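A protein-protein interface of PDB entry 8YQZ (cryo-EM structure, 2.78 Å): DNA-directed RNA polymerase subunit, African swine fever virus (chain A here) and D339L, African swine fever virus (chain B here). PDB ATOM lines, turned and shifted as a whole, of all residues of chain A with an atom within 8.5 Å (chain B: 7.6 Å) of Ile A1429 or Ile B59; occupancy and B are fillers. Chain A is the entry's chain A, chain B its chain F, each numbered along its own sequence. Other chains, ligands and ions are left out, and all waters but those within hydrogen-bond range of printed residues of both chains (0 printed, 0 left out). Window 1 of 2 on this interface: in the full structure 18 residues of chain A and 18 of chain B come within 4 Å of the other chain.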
ATOM      1  N   TYR A   5      14.448  -1.697  -3.060  1.00  0.00           N
ATOM      2  CA  TYR A   5      15.718  -1.023  -3.294  1.00  0.00           C
ATOM      3  C   TYR A   5      15.826   0.237  -2.445  1.00  0.00           C
ATOM      4  O   TYR A   5      14.885   1.031  -2.375  1.00  0.00           O
ATOM      5  CB  TYR A   5      15.837  -0.680  -4.775  1.00  0.00           C
ATOM      6  CG  TYR A   5      17.011   0.178  -5.156  1.00  0.00           C
ATOM      7  CD1 TYR A   5      18.225  -0.381  -5.489  1.00  0.00           C
ATOM      8  CD2 TYR A   5      16.902   1.552  -5.187  1.00  0.00           C
ATOM      9  CE1 TYR A   5      19.286   0.407  -5.839  1.00  0.00           C
ATOM     10  CE2 TYR A   5      17.952   2.335  -5.527  1.00  0.00           C
ATOM     11  CZ  TYR A   5      19.138   1.763  -5.859  1.00  0.00           C
ATOM     12  OH  TYR A   5      20.188   2.564  -6.204  1.00  0.00           O
ATOM     13  N   GLU A   7      18.842   3.315  -0.623  1.00  0.00           N
ATOM     14  CA  GLU A   7      20.170   3.910  -0.552  1.00  0.00           C
ATOM     15  C   GLU A   7      20.381   4.519   0.822  1.00  0.00           C
ATOM     16  O   GLU A   7      19.434   4.999   1.441  1.00  0.00           O
ATOM     17  CB  GLU A   7      20.368   4.987  -1.615  1.00  0.00           C
ATOM     18  CG  GLU A   7      20.683   4.462  -2.991  1.00  0.00           C
ATOM     19  CD  GLU A   7      20.086   5.316  -4.082  1.00  0.00           C
ATOM     20  OE1 GLU A   7      19.109   6.035  -3.803  1.00  0.00           O
ATOM     21  OE2 GLU A   7      20.585   5.268  -5.222  1.00  0.00           O
ATOM     22  N   MET A 472      26.331  -1.639 -19.849  1.00  0.00           N
ATOM     23  CA  MET A 472      26.407  -0.292 -19.298  1.00  0.00           C
ATOM     24  C   MET A 472      27.839   0.209 -19.230  1.00  0.00           C
ATOM     25  O   MET A 472      28.097   1.392 -19.460  1.00  0.00           O
ATOM     26  CB  MET A 472      25.769  -0.253 -17.916  1.00  0.00           C
ATOM     27  CG  MET A 472      24.276  -0.150 -17.945  1.00  0.00           C
ATOM     28  SD  MET A 472      23.642   0.630 -16.468  1.00  0.00           S
ATOM     29  CE  MET A 472      21.927   0.218 -16.591  1.00  0.00           C
ATOM     30  N   TYR A 840      23.766  22.234 -10.652  1.00  0.00           N
ATOM     31  CA  TYR A 840      22.872  22.528 -11.762  1.00  0.00           C
ATOM     32  C   TYR A 840      22.836  24.002 -12.115  1.00  0.00           C
ATOM     33  O   TYR A 840      22.151  24.380 -13.065  1.00  0.00           O
ATOM     34  CB  TYR A 840      21.457  22.068 -11.439  1.00  0.00           C
ATOM     35  CG  TYR A 840      21.284  20.589 -11.576  1.00  0.00           C
ATOM     36  CD1 TYR A 840      21.538  19.957 -12.768  1.00  0.00           C
ATOM     37  CD2 TYR A 840      20.879  19.824 -10.502  1.00  0.00           C
ATOM     38  CE1 TYR A 840      21.396  18.612 -12.887  1.00  0.00           C
ATOM     39  CE2 TYR A 840      20.739  18.479 -10.614  1.00  0.00           C
ATOM     40  CZ  TYR A 840      20.994  17.875 -11.807  1.00  0.00           C
ATOM     41  OH  TYR A 840      20.845  16.524 -11.917  1.00  0.00           O
ATOM     42  N   ARG A1421      27.566   9.915  -6.245  1.00  0.00           N
ATOM     43  CA  ARG A1421      26.516  10.480  -7.090  1.00  0.00           C
ATOM     44  C   ARG A1421      27.107  11.608  -7.913  1.00  0.00           C
ATOM     45  O   ARG A1421      26.944  12.782  -7.605  1.00  0.00           O
ATOM     46  CB  ARG A1421      25.359  10.978  -6.244  1.00  0.00           C
ATOM     47  CG  ARG A1421      24.126  11.285  -7.034  1.00  0.00           C
ATOM     48  CD  ARG A1421      23.083  11.943  -6.171  1.00  0.00           C
ATOM     49  NE  ARG A1421      22.562  11.021  -5.170  1.00  0.00           N
ATOM     50  CZ  ARG A1421      21.644  10.097  -5.408  1.00  0.00           C
ATOM     51  NH1 ARG A1421      21.117   9.940  -6.608  1.00  0.00           N
ATOM     52  NH2 ARG A1421      21.244   9.312  -4.414  1.00  0.00           N
ATOM     53  N   THR A1424      28.166  10.320 -14.609  1.00  0.00           N
ATOM     54  CA  THR A1424      26.992   9.749 -15.256  1.00  0.00           C
ATOM     55  C   THR A1424      25.892   9.452 -14.255  1.00  0.00           C
ATOM     56  O   THR A1424      24.746   9.253 -14.652  1.00  0.00           O
ATOM     57  CB  THR A1424      27.355   8.479 -16.032  1.00  0.00           C
ATOM     58  OG1 THR A1424      28.211   7.648 -15.247  1.00  0.00           O
ATOM     59  CG2 THR A1424      28.056   8.821 -17.326  1.00  0.00           C
ATOM     60  N   MET A1425      26.209   9.463 -12.967  1.00  0.00           N
ATOM     61  CA  MET A1425      25.256   9.159 -11.917  1.00  0.00           C
ATOM     62  C   MET A1425      24.730  10.395 -11.212  1.00  0.00           C
ATOM     63  O   MET A1425      24.138  10.277 -10.143  1.00  0.00           O
ATOM     64  CB  MET A1425      25.886   8.204 -10.913  1.00  0.00           C
ATOM     65  CG  MET A1425      25.025   7.001 -10.699  1.00  0.00           C
ATOM     66  SD  MET A1425      25.278   5.652 -11.832  1.00  0.00           S
ATOM     67  CE  MET A1425      26.685   4.896 -11.073  1.00  0.00           C
ATOM     68  N   TYR A1426      24.917  11.574 -11.793  1.00  0.00           N
ATOM     69  CA  TYR A1426      24.505  12.795 -11.125  1.00  0.00           C
ATOM     70  C   TYR A1426      23.010  13.039 -11.261  1.00  0.00           C
ATOM     71  O   TYR A1426      22.371  13.524 -10.326  1.00  0.00           O
ATOM     72  CB  TYR A1426      25.295  13.975 -11.673  1.00  0.00           C
ATOM     73  CG  TYR A1426      25.120  15.232 -10.880  1.00  0.00           C
ATOM     74  CD1 TYR A1426      25.615  15.337  -9.599  1.00  0.00           C
ATOM     75  CD2 TYR A1426      24.446  16.310 -11.407  1.00  0.00           C
ATOM     76  CE1 TYR A1426      25.443  16.473  -8.878  1.00  0.00           C
ATOM     77  CE2 TYR A1426      24.275  17.452 -10.687  1.00  0.00           C
ATOM     78  CZ  TYR A1426      24.772  17.527  -9.423  1.00  0.00           C
ATOM     79  OH  TYR A1426      24.606  18.661  -8.688  1.00  0.00           O
ATOM     80  N   SER A1427      22.438  12.731 -12.413  1.00  0.00           N
ATOM     81  CA  SER A1427      21.033  12.988 -12.680  1.00  0.00           C
ATOM     82  C   SER A1427      20.252  11.684 -12.693  1.00  0.00           C
ATOM     83  O   SER A1427      20.737  10.667 -13.190  1.00  0.00           O
ATOM     84  CB  SER A1427      20.848  13.709 -14.013  1.00  0.00           C
ATOM     85  OG  SER A1427      21.285  15.048 -13.937  1.00  0.00           O
ATOM     86  N   ASP A1428      19.046  11.724 -12.141  1.00  0.00           N
ATOM     87  CA  ASP A1428      18.155  10.577 -12.119  1.00  0.00           C
ATOM     88  C   ASP A1428      17.540  10.349 -13.490  1.00  0.00           C
ATOM     89  O   ASP A1428      17.326  11.291 -14.253  1.00  0.00           O
ATOM     90  CB  ASP A1428      17.044  10.785 -11.095  1.00  0.00           C
ATOM     91  CG  ASP A1428      17.256   9.987  -9.836  1.00  0.00           C
ATOM     92  OD1 ASP A1428      17.760   8.851  -9.920  1.00  0.00           O
ATOM     93  OD2 ASP A1428      16.913  10.492  -8.750  1.00  0.00           O
ATOM     94  N   ILE A1429      17.260   9.089 -13.798  1.00  0.00           N
ATOM     95  CA  ILE A1429      16.511   8.709 -14.989  1.00  0.00           C
ATOM     96  C   ILE A1429      15.207   8.073 -14.532  1.00  0.00           C
ATOM     97  O   ILE A1429      15.198   7.269 -13.597  1.00  0.00           O
ATOM     98  CB  ILE A1429      17.317   7.746 -15.878  1.00  0.00           C
ATOM     99  CG1 ILE A1429      18.696   8.319 -16.219  1.00  0.00           C
ATOM    100  CG2 ILE A1429      16.560   7.419 -17.135  1.00  0.00           C
ATOM    101  CD1 ILE A1429      18.684   9.610 -16.992  1.00  0.00           C
ATOM    102  N   ILE A1430      14.100   8.460 -15.156  1.00  0.00           N
ATOM    103  CA  ILE A1430      12.806   7.846 -14.903  1.00  0.00           C
ATOM    104  C   ILE A1430      12.196   7.441 -16.235  1.00  0.00           C
ATOM    105  O   ILE A1430      12.553   7.957 -17.292  1.00  0.00           O
ATOM    106  CB  ILE A1430      11.849   8.770 -14.123  1.00  0.00           C
ATOM    107  CG1 ILE A1430      11.508  10.005 -14.943  1.00  0.00           C
ATOM    108  CG2 ILE A1430      12.443   9.163 -12.799  1.00  0.00           C
ATOM    109  CD1 ILE A1430      10.519  10.897 -14.287  1.00  0.00           C
ATOM    110  N   MET A1431      11.272   6.493 -16.179  1.00  0.00           N
ATOM    111  CA  MET A1431      10.679   5.947 -17.389  1.00  0.00           C
ATOM    112  C   MET A1431       9.555   6.859 -17.857  1.00  0.00           C
ATOM    113  O   MET A1431       8.790   7.380 -17.041  1.00  0.00           O
ATOM    114  CB  MET A1431      10.163   4.530 -17.156  1.00  0.00           C
ATOM    115  CG  MET A1431      11.214   3.600 -16.596  1.00  0.00           C
ATOM    116  SD  MET A1431      12.210   2.728 -17.808  1.00  0.00           S
ATOM    117  CE  MET A1431      11.055   2.484 -19.129  1.00  0.00           C
ATOM    118  N   ASP A1432       9.473   7.065 -19.165  1.00  0.00           N
ATOM    119  CA  ASP A1432       8.483   7.948 -19.777  1.00  0.00           C
ATOM    120  C   ASP A1432       7.187   7.172 -19.982  1.00  0.00           C
ATOM    121  O   ASP A1432       6.959   6.561 -21.024  1.00  0.00           O
ATOM    122  CB  ASP A1432       9.023   8.500 -21.084  1.00  0.00           C
ATOM    123  CG  ASP A1432       8.279   9.712 -21.558  1.00  0.00           C
ATOM    124  OD1 ASP A1432       7.241  10.059 -20.959  1.00  0.00           O
ATOM    125  OD2 ASP A1432       8.732  10.323 -22.542  1.00  0.00           O
ATOM    126  N   ILE B  13      11.043  -3.457  -9.912  1.00  0.00           N
ATOM    127  CA  ILE B  13      10.485  -3.761 -11.224  1.00  0.00           C
ATOM    128  C   ILE B  13      11.592  -4.363 -12.072  1.00  0.00           C
ATOM    129  O   ILE B  13      12.611  -3.713 -12.322  1.00  0.00           O
ATOM    130  CB  ILE B  13       9.898  -2.511 -11.893  1.00  0.00           C
ATOM    131  CG1 ILE B  13       8.631  -2.064 -11.180  1.00  0.00           C
ATOM    132  CG2 ILE B  13       9.601  -2.772 -13.332  1.00  0.00           C
ATOM    133  CD1 ILE B  13       8.795  -0.874 -10.348  1.00  0.00           C
ATOM    134  N   PRO B  16      11.057  -2.633 -16.639  1.00  0.00           N
ATOM    135  CA  PRO B  16      10.364  -1.335 -16.600  1.00  0.00           C
ATOM    136  C   PRO B  16       9.619  -0.975 -17.876  1.00  0.00           C
ATOM    137  O   PRO B  16       8.559  -0.343 -17.805  1.00  0.00           O
ATOM    138  CB  PRO B  16      11.505  -0.356 -16.304  1.00  0.00           C
ATOM    139  CG  PRO B  16      12.555  -1.178 -15.677  1.00  0.00           C
ATOM    140  CD  PRO B  16      12.489  -2.496 -16.343  1.00  0.00           C
ATOM    141  N   THR B  17      10.139  -1.354 -19.043  1.00  0.00           N
ATOM    142  CA  THR B  17       9.470  -0.995 -20.289  1.00  0.00           C
ATOM    143  C   THR B  17       8.107  -1.665 -20.392  1.00  0.00           C
ATOM    144  O   THR B  17       7.132  -1.044 -20.827  1.00  0.00           O
ATOM    145  CB  THR B  17      10.338  -1.379 -21.484  1.00  0.00           C
ATOM    146  OG1 THR B  17      11.719  -1.240 -21.138  1.00  0.00           O
ATOM    147  CG2 THR B  17      10.050  -0.464 -22.646  1.00  0.00           C
ATOM    148  N   PRO B  56       7.203   8.071  -9.507  1.00  0.00           N
ATOM    149  CA  PRO B  56       7.606   7.596 -10.835  1.00  0.00           C
ATOM    150  C   PRO B  56       8.403   6.301 -10.746  1.00  0.00           C
ATOM    151  O   PRO B  56       8.744   5.821  -9.667  1.00  0.00           O
ATOM    152  CB  PRO B  56       8.468   8.739 -11.372  1.00  0.00           C
ATOM    153  CG  PRO B  56       7.999   9.920 -10.650  1.00  0.00           C
ATOM    154  CD  PRO B  56       7.606   9.470  -9.291  1.00  0.00           C
ATOM    155  N   CYS B  57       8.693   5.729 -11.906  1.00  0.00           N
ATOM    156  CA  CYS B  57       9.521   4.528 -11.960  1.00  0.00           C
ATOM    157  C   CYS B  57      10.975   4.955 -12.130  1.00  0.00           C
ATOM    158  O   CYS B  57      11.429   5.272 -13.224  1.00  0.00           O
ATOM    159  CB  CYS B  57       9.064   3.606 -13.083  1.00  0.00           C
ATOM    160  SG  CYS B  57       9.901   2.010 -13.130  1.00  0.00           S
ATOM    161  N   PHE B  58      11.706   4.985 -11.024  1.00  0.00           N
ATOM    162  CA  PHE B  58      13.118   5.317 -11.061  1.00  0.00           C
ATOM    163  C   PHE B  58      13.946   4.121 -11.503  1.00  0.00           C
ATOM    164  O   PHE B  58      13.642   2.978 -11.178  1.00  0.00           O
ATOM    165  CB  PHE B  58      13.607   5.771  -9.690  1.00  0.00           C
ATOM    166  CG  PHE B  58      12.778   6.848  -9.061  1.00  0.00           C
ATOM    167  CD1 PHE B  58      12.802   8.132  -9.556  1.00  0.00           C
ATOM    168  CD2 PHE B  58      12.012   6.587  -7.951  1.00  0.00           C
ATOM    169  CE1 PHE B  58      12.061   9.121  -8.978  1.00  0.00           C
ATOM    170  CE2 PHE B  58      11.277   7.576  -7.366  1.00  0.00           C
ATOM    171  CZ  PHE B  58      11.300   8.846  -7.881  1.00  0.00           C
ATOM    172  N   ILE B  59      15.018   4.398 -12.225  1.00  0.00           N
ATOM    173  CA  ILE B  59      15.970   3.371 -12.625  1.00  0.00           C
ATOM    174  C   ILE B  59      16.986   3.199 -11.512  1.00  0.00           C
ATOM    175  O   ILE B  59      17.448   4.181 -10.930  1.00  0.00           O
ATOM    176  CB  ILE B  59      16.649   3.730 -13.956  1.00  0.00           C
ATOM    177  CG1 ILE B  59      15.595   4.070 -15.000  1.00  0.00           C
ATOM    178  CG2 ILE B  59      17.502   2.578 -14.446  1.00  0.00           C
ATOM    179  CD1 ILE B  59      14.584   2.983 -15.194  1.00  0.00           C
ATOM    180  N   MET B  60      17.319   1.951 -11.203  1.00  0.00           N
ATOM    181  CA  MET B  60      18.270   1.669 -10.137  1.00  0.00           C
ATOM    182  C   MET B  60      19.626   2.267 -10.470  1.00  0.00           C
ATOM    183  O   MET B  60      20.043   2.299 -11.627  1.00  0.00           O
ATOM    184  CB  MET B  60      18.388   0.167  -9.924  1.00  0.00           C
ATOM    185  CG  MET B  60      17.278  -0.416  -9.093  1.00  0.00           C
ATOM    186  SD  MET B  60      17.524  -2.155  -8.738  1.00  0.00           S
ATOM    187  CE  MET B  60      15.844  -2.735  -8.693  1.00  0.00           C
ATOM    188  N   ARG B  61      20.313   2.749  -9.446  1.00  0.00           N
ATOM    189  CA  ARG B  61      21.466   3.611  -9.628  1.00  0.00           C
ATOM    190  C   ARG B  61      22.773   3.000  -9.148  1.00  0.00           C
ATOM    191  O   ARG B  61      23.833   3.422  -9.607  1.00  0.00           O
ATOM    192  CB  ARG B  61      21.226   4.926  -8.889  1.00  0.00           C
ATOM    193  CG  ARG B  61      22.034   6.093  -9.345  1.00  0.00           C
ATOM    194  CD  ARG B  61      22.190   7.100  -8.227  1.00  0.00           C
ATOM    195  NE  ARG B  61      23.542   7.105  -7.682  1.00  0.00           N
ATOM    196  CZ  ARG B  61      23.847   6.883  -6.413  1.00  0.00           C
ATOM    197  NH1 ARG B  61      22.914   6.653  -5.507  1.00  0.00           N
ATOM    198  NH2 ARG B  61      25.122   6.886  -6.044  1.00  0.00           N
ATOM    199  N   THR B  62      22.735   2.029  -8.245  1.00  0.00           N
ATOM    200  CA  THR B  62      23.941   1.496  -7.633  1.00  0.00           C
ATOM    201  C   THR B  62      24.373   0.166  -8.225  1.00  0.00           C
ATOM    202  O   THR B  62      25.263  -0.483  -7.676  1.00  0.00           O
ATOM    203  CB  THR B  62      23.754   1.366  -6.123  1.00  0.00           C
ATOM    204  OG1 THR B  62      22.611   0.552  -5.853  1.00  0.00           O
ATOM    205  CG2 THR B  62      23.570   2.723  -5.482  1.00  0.00           C
ATOM    206  N   ASN B  63      23.771  -0.250  -9.332  1.00  0.00           N
ATOM    207  CA  ASN B  63      24.197  -1.447 -10.035  1.00  0.00           C
ATOM    208  C   ASN B  63      23.838  -1.285 -11.501  1.00  0.00           C
ATOM    209  O   ASN B  63      23.088  -0.384 -11.877  1.00  0.00           O
ATOM    210  CB  ASN B  63      23.566  -2.710  -9.446  1.00  0.00           C
ATOM    211  CG  ASN B  63      22.073  -2.640  -9.385  1.00  0.00           C
ATOM    212  OD1 ASN B  63      21.469  -1.679  -9.821  1.00  0.00           O
ATOM    213  ND2 ASN B  63      21.467  -3.651  -8.819  1.00  0.00           N
ATOM    214  N   SER B  65      22.126  -3.256 -13.490  1.00  0.00           N
ATOM    215  CA  SER B  65      21.054  -4.146 -13.916  1.00  0.00           C
ATOM    216  C   SER B  65      20.038  -3.485 -14.834  1.00  0.00           C
ATOM    217  O   SER B  65      19.402  -4.185 -15.620  1.00  0.00           O
ATOM    218  CB  SER B  65      20.339  -4.722 -12.698  1.00  0.00           C
ATOM    219  OG  SER B  65      19.806  -3.703 -11.887  1.00  0.00           O
ATOM    220  N   GLY B  66      19.867  -2.171 -14.763  1.00  0.00           N
ATOM    221  CA  GLY B  66      18.875  -1.511 -15.587  1.00  0.00           C
ATOM    222  C   GLY B  66      17.457  -1.672 -15.107  1.00  0.00           C
ATOM    223  O   GLY B  66      16.523  -1.445 -15.872  1.00  0.00           O
ATOM    224  N   ARG B  67      17.273  -2.050 -13.852  1.00  0.00           N
ATOM    225  CA  ARG B  67      15.977  -2.363 -13.280  1.00  0.00           C
ATOM    226  C   ARG B  67      15.385  -1.127 -12.615  1.00  0.00           C
ATOM    227  O   ARG B  67      16.085  -0.163 -12.312  1.00  0.00           O
ATOM    228  CB  ARG B  67      16.112  -3.497 -12.270  1.00  0.00           C
ATOM    229  CG  ARG B  67      16.012  -4.872 -12.868  1.00  0.00           C
ATOM    230  CD  ARG B  67      16.131  -5.932 -11.801  1.00  0.00           C
ATOM    231  NE  ARG B  67      17.337  -5.781 -11.005  1.00  0.00           N
ATOM    232  CZ  ARG B  67      17.447  -6.140  -9.735  1.00  0.00           C
ATOM    233  NH1 ARG B  67      16.423  -6.646  -9.069  1.00  0.00           N
ATOM    234  NH2 ARG B  67      18.610  -5.977  -9.115  1.00  0.00           N
ATOM    235  N   GLY B  68      14.075  -1.165 -12.389  1.00  0.00           N
ATOM    236  CA  GLY B  68      13.349  -0.046 -11.840  1.00  0.00           C
ATOM    237  C   GLY B  68      12.913  -0.294 -10.407  1.00  0.00           C
ATOM    238  O   GLY B  68      13.053  -1.381  -9.860  1.00  0.00           O
ATOM    239  N   TYR B  69      12.397   0.759  -9.791  1.00  0.00           N
ATOM    240  CA  TYR B  69      11.763   0.628  -8.492  1.00  0.00           C
ATOM    241  C   TYR B  69      10.737   1.734  -8.342  1.00  0.00           C
ATOM    242  O   TYR B  69      10.799   2.756  -9.026  1.00  0.00           O
ATOM    243  CB  TYR B  69      12.783   0.639  -7.342  1.00  0.00           C
ATOM    244  CG  TYR B  69      13.533   1.933  -7.146  1.00  0.00           C
ATOM    245  CD1 TYR B  69      14.663   2.213  -7.891  1.00  0.00           C
ATOM    246  CD2 TYR B  69      13.132   2.860  -6.195  1.00  0.00           C
ATOM    247  CE1 TYR B  69      15.350   3.381  -7.719  1.00  0.00           C
ATOM    248  CE2 TYR B  69      13.818   4.027  -6.018  1.00  0.00           C
ATOM    249  CZ  TYR B  69      14.927   4.283  -6.784  1.00  0.00           C
ATOM    250  OH  TYR B  69      15.632   5.446  -6.618  1.00  0.00           O
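O of Cys B57 lies within hydrogen-bond range of N of Met A1431 (3.2 Å).
The side-chain hydroxyl (OH) of Tyr A5 lies within hydrogen-bond range of the backbone NH (N) of Arg B61.
The guanidinium group (NH2) of Arg A1421 sits close to the guanidinium group (NH1) of Arg B61, 3.3 Å away.
OE2 of Glu A7 lies within salt-bridge range of NH1 of Arg B61, at 2.7 Å.
OH of Tyr A5 sits at hydrogen-bond distance from OG1 of Thr B62, 3.2 Å away.
N of Ile B59 lies within hydrogen-bond range of O of Ile A1429, 3.2 Å away.
The side-chain sulfur (SD) of Met A1425 lies close to the backbone carbonyl oxygen (O) of Arg B61 (3.5 Å).
Of chain B, only Phe B58 and Ile B59 come within 4 Å of Ile A1429.
Of the printed residues of chain A, Ile B59 touches Ile A1429 (3.2 Å) and Met A1431 (3.5 Å).
Of the printed residues of chain A, Gly B66 touches Met A472 (3.6 Å).
Of the printed residues of chain A, Phe B58 touches Ile A1429 and Ile A1430.
Of the printed residues of chain B, Tyr A5 touches Met B60 (3.7 Å), Arg B61 (3.2 Å), Thr B62 (3.2 Å) and Tyr B69 (3.5 Å).
Printed residues of chain B within 4 Å of Met A1431: Pro B16, Thr B17, Cys B57 and Ile B59.
Of the printed residues of chain A, Cys B57 touches Ile A1430 and Met A1431.
Asp A1428 touches none of the printed residues of chain B.
The backbone carbonyl oxygen (O) of Arg B67 lies within hydrogen-bond range of the backbone NH (N) of Met B60, at 2.7 Å.
OH of Tyr A5 lies within hydrogen-bond range of OE2 of Glu A7, 2.9 Å away.
The side-chain carboxylate of Glu A7 lies within salt-bridge range of the guanidinium group of Arg A1421.
The backbone carbonyl oxygen (O) of Phe B58 lies within hydrogen-bond range of the backbone NH (N) of Tyr B69 (2.9 Å).
Among the printed residues, merely in contact across the chains: Tyr A5 with Met B60 (3.7 Å), Tyr A5 with Tyr B69 (3.5 Å), Glu A7 with Thr B62 (3.9 Å), Met A472 with Gly B66 (3.6 Å), Ile A1429 with Phe B58 (3.8 Å), Ile A1430 with Cys B57 (3.4 Å), Ile A1430 with Phe B58 (3.4 Å), Met A1431 with Pro B16 (3.5 Å), Met A1431 with Thr B17 (3.9 Å) and Met A1431 with Ile B59 (3.5 Å).
Of the 14 printed residues of chain A, 8 touch a printed residue of chain B.
Hydrophobic or aromatic side chains of chain A that line the printed part of chain B: Tyr A5, Met A472, Met A1425, Ile A1430 and Met A1431.
Of the 16 printed residues of chain B, 10 touch a printed residue of chain A.
Printed residues of chain B that touch a printed residue of chain A: Pro B16, Thr B17, Cys B57, Phe B58, Ile B59, Met B60, Arg B61, Thr B62, Gly B66 and Tyr B69.
Hydrophobic or aromatic side chains of chain B within 4 Å of the printed part of chain A: Pro B16, Phe B58, Ile B59, Met B60 and Tyr B69.
Along chain B the printed residues that touch a printed residue of chain A span positions 16 to 69.
Among the printed residues, Asp or Glu carboxylates within 4 Å of a Lys or Arg side-chain nitrogen of the other chain: Glu A7 with Arg B61.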
